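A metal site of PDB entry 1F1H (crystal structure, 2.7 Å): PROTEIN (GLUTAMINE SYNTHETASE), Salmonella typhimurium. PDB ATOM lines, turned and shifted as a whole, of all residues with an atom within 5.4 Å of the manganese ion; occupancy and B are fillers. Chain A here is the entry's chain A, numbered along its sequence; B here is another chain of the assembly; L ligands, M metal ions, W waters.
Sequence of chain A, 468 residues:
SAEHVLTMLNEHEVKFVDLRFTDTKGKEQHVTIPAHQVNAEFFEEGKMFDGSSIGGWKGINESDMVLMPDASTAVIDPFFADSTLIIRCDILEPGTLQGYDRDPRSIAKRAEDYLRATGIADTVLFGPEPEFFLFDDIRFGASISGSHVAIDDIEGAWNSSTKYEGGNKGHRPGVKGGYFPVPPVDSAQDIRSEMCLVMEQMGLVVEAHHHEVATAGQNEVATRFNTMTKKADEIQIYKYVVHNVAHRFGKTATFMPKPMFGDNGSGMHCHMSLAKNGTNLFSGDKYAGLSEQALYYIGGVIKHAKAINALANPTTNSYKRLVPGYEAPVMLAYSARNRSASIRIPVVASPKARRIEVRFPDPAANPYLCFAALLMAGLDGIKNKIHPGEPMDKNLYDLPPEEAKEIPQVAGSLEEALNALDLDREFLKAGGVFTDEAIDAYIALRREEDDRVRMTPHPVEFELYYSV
The side-chain carboxylate (OE2) of Glu 220 sits close to an oxygen (O1) of the ligand (2.9 Å).
O2 of the ligand is in hydrogen-bond range of NE2 of His 210, 2.8 Å away.
The side-chain carboxylate (OD2) of Asp 50 of chain B sits close to an oxygen (O3) of the ligand, at 2.9 Å.
O of His 210 sits at hydrogen-bond distance from N of Glu 220 (2.9 Å).
Of the 7 residues printed, 3 come within 4 Å of the manganese ion.
The manganese ion is bound by OE1 of Glu 131 (2.0 Å), water W2 (2.1 Å), OE1 of Glu 220 (2.2 Å), water W1 (2.2 Å) and OE2 of Glu 212 (2.3 Å).
Water W1 lies within hydrogen-bond range of an oxygen (O1) of the ligand (2.5 Å) and the side-chain carboxylate (OE2) of Glu 220 (3.0 Å).
Water W2 bridges O1 of the ligand and OD2 of Asp 50 of chain B.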
ATOM      1  N   GLU A 131      14.630  13.264 -14.902  1.00  0.00           N
ATOM      2  CA  GLU A 131      15.399  14.496 -14.767  1.00  0.00           C
ATOM      3  C   GLU A 131      16.769  14.262 -14.147  1.00  0.00           C
ATOM      4  O   GLU A 131      16.981  13.261 -13.457  1.00  0.00           O
ATOM      5  CB  GLU A 131      14.618  15.495 -13.923  1.00  0.00           C
ATOM      6  CG  GLU A 131      13.465  16.113 -14.672  1.00  0.00           C
ATOM      7  CD  GLU A 131      12.416  16.709 -13.767  1.00  0.00           C
ATOM      8  OE1 GLU A 131      11.626  17.552 -14.248  1.00  0.00           O
ATOM      9  OE2 GLU A 131      12.367  16.317 -12.567  1.00  0.00           O
ATOM     10  N   TYR A 179      14.664  27.964 -15.100  1.00  0.00           N
ATOM     11  CA  TYR A 179      13.715  27.520 -16.078  1.00  0.00           C
ATOM     12  C   TYR A 179      13.604  28.426 -17.238  1.00  0.00           C
ATOM     13  O   TYR A 179      13.118  29.547 -17.177  1.00  0.00           O
ATOM     14  CB  TYR A 179      12.420  27.222 -15.425  1.00  0.00           C
ATOM     15  CG  TYR A 179      11.832  25.956 -15.977  1.00  0.00           C
ATOM     16  CD1 TYR A 179      12.578  24.825 -16.393  1.00  0.00           C
ATOM     17  CD2 TYR A 179      10.455  25.889 -16.111  1.00  0.00           C
ATOM     18  CE1 TYR A 179      11.964  23.692 -16.889  1.00  0.00           C
ATOM     19  CE2 TYR A 179       9.824  24.746 -16.601  1.00  0.00           C
ATOM     20  CZ  TYR A 179      10.588  23.667 -16.981  1.00  0.00           C
ATOM     21  OH  TYR A 179       9.977  22.550 -17.471  1.00  0.00           O
ATOM     22  N   HIS A 210      15.492  20.539 -22.471  1.00  0.00           N
ATOM     23  CA  HIS A 210      15.444  21.835 -21.850  1.00  0.00           C
ATOM     24  C   HIS A 210      16.085  21.814 -20.484  1.00  0.00           C
ATOM     25  O   HIS A 210      16.287  20.746 -19.901  1.00  0.00           O
ATOM     26  CB  HIS A 210      13.983  22.253 -21.678  1.00  0.00           C
ATOM     27  CG  HIS A 210      13.157  21.270 -20.887  1.00  0.00           C
ATOM     28  ND1 HIS A 210      13.017  21.356 -19.514  1.00  0.00           N
ATOM     29  CD2 HIS A 210      12.439  20.190 -21.270  1.00  0.00           C
ATOM     30  CE1 HIS A 210      12.242  20.377 -19.091  1.00  0.00           C
ATOM     31  NE2 HIS A 210      11.876  19.651 -20.138  1.00  0.00           N
ATOM     32  N   GLU A 212      16.035  22.536 -16.483  1.00  0.00           N
ATOM     33  CA  GLU A 212      14.954  22.368 -15.528  1.00  0.00           C
ATOM     34  C   GLU A 212      14.930  23.493 -14.522  1.00  0.00           C
ATOM     35  O   GLU A 212      15.692  24.439 -14.629  1.00  0.00           O
ATOM     36  CB  GLU A 212      15.031  21.011 -14.837  1.00  0.00           C
ATOM     37  CG  GLU A 212      14.036  19.985 -15.345  1.00  0.00           C
ATOM     38  CD  GLU A 212      12.583  20.352 -15.036  1.00  0.00           C
ATOM     39  OE1 GLU A 212      12.313  20.991 -13.985  1.00  0.00           O
ATOM     40  OE2 GLU A 212      11.702  19.973 -15.844  1.00  0.00           O
ATOM     41  N   GLU A 220      16.891  18.210 -18.540  1.00  0.00           N
ATOM     42  CA  GLU A 220      16.015  17.120 -18.930  1.00  0.00           C
ATOM     43  C   GLU A 220      15.969  16.873 -20.414  1.00  0.00           C
ATOM     44  O   GLU A 220      15.977  17.814 -21.218  1.00  0.00           O
ATOM     45  CB  GLU A 220      14.595  17.396 -18.448  1.00  0.00           C
ATOM     46  CG  GLU A 220      13.727  16.156 -18.497  1.00  0.00           C
ATOM     47  CD  GLU A 220      12.279  16.393 -18.094  1.00  0.00           C
ATOM     48  OE1 GLU A 220      11.972  17.318 -17.296  1.00  0.00           O
ATOM     49  OE2 GLU A 220      11.437  15.630 -18.573  1.00  0.00           O
ATOM     50  N   HIS A 269       8.454  11.192 -13.654  1.00  0.00           N
ATOM     51  CA  HIS A 269       7.029  10.974 -13.877  1.00  0.00           C
ATOM     52  C   HIS A 269       6.893   9.795 -14.837  1.00  0.00           C
ATOM     53  O   HIS A 269       7.724   9.608 -15.737  1.00  0.00           O
ATOM     54  CB  HIS A 269       6.353  12.188 -14.526  1.00  0.00           C
ATOM     55  CG  HIS A 269       6.448  13.464 -13.750  1.00  0.00           C
ATOM     56  ND1 HIS A 269       6.227  14.701 -14.329  1.00  0.00           N
ATOM     57  CD2 HIS A 269       6.716  13.706 -12.446  1.00  0.00           C
ATOM     58  CE1 HIS A 269       6.368  15.648 -13.417  1.00  0.00           C
ATOM     59  NE2 HIS A 269       6.665  15.071 -12.262  1.00  0.00           N
ATOM     60  N   ASP B  50       4.181  21.760 -19.204  1.00  0.00           N
ATOM     61  CA  ASP B  50       3.945  21.503 -17.736  1.00  0.00           C
ATOM     62  C   ASP B  50       4.284  22.826 -17.022  1.00  0.00           C
ATOM     63  O   ASP B  50       4.867  22.916 -15.934  1.00  0.00           O
ATOM     64  CB  ASP B  50       4.673  20.257 -17.238  1.00  0.00           C
ATOM     65  CG  ASP B  50       6.139  20.453 -16.702  1.00  0.00           C
ATOM     66  OD1 ASP B  50       6.315  20.718 -15.512  1.00  0.00           O
ATOM     67  OD2 ASP B  50       7.082  20.362 -17.533  1.00  0.00           O
HETATM   68  P1  LIG L   1       8.663  17.040 -19.390  1.00  0.00           P
HETATM   69  O1  LIG L   1       8.771  16.454 -17.952  1.00  0.00           O
HETATM   70  O2  LIG L   1       9.879  17.659 -19.939  1.00  0.00           O
HETATM   71  O3  LIG L   1       7.363  18.108 -19.350  1.00  0.00           O
HETATM   72  P2  LIG L   1       6.767  15.608 -21.357  1.00  0.00           P
HETATM   73  O4  LIG L   1       5.522  16.312 -20.807  1.00  0.00           O
HETATM   74  O5  LIG L   1       7.122  16.157 -22.774  1.00  0.00           O
HETATM   75  O6  LIG L   1       8.059  15.772 -20.295  1.00  0.00           O
HETATM   76  O7  LIG L   1       6.237  14.093 -21.460  1.00  0.00           O
HETATM   77  C1  LIG L   1       6.417  12.969 -22.308  1.00  0.00           C
HETATM   78  C2  LIG L   1       6.031  11.553 -22.286  1.00  0.00           C
HETATM   79  O8  LIG L   1       4.590  11.020 -22.312  1.00  0.00           O
HETATM   80  C3  LIG L   1       6.621  11.092 -23.541  1.00  0.00           C
HETATM   81  O9  LIG L   1       7.707  10.251 -23.195  1.00  0.00           O
HETATM   82  C4  LIG L   1       5.361  10.531 -24.248  1.00  0.00           C
HETATM   83  O10 LIG L   1       5.735   9.931 -25.456  1.00  0.00           O
HETATM   84  C5  LIG L   1       4.801   9.732 -23.084  1.00  0.00           C
HETATM   85  N1  LIG L   1       3.481   8.693 -23.386  1.00  0.00           N
HETATM   86  C6  LIG L   1       3.157   7.502 -22.592  1.00  0.00           C
HETATM   87  N2  LIG L   1       2.114   6.755 -22.918  1.00  0.00           N
HETATM   88  C7  LIG L   1       1.632   7.444 -24.011  1.00  0.00           C
HETATM   89  C8  LIG L   1       0.516   7.161 -24.827  1.00  0.00           C
HETATM   90  N3  LIG L   1      -0.144   6.154 -24.578  1.00  0.00           N
HETATM   91  N4  LIG L   1       0.197   7.952 -25.873  1.00  0.00           N
HETATM   92  C9  LIG L   1       0.951   9.046 -26.121  1.00  0.00           C
HETATM   93  N5  LIG L   1       2.072   9.499 -25.443  1.00  0.00           N
HETATM   94  C10 LIG L   1       2.393   8.628 -24.356  1.00  0.00           C
HETATM   95 MN    MN M   1      10.459  18.030 -15.831  1.00  0.00          MN
HETATM   96 TL    TL M   2       9.365  21.551 -14.880  1.00  0.00          TL
HETATM   97 TL    TL M   3      11.441  18.204 -10.916  1.00  0.00          TL
HETATM   98  O   HOH W   1      10.113  15.832 -15.896  1.00  0.00           O
HETATM   99  O   HOH W   2       9.485  18.978 -17.393  1.00  0.00           O
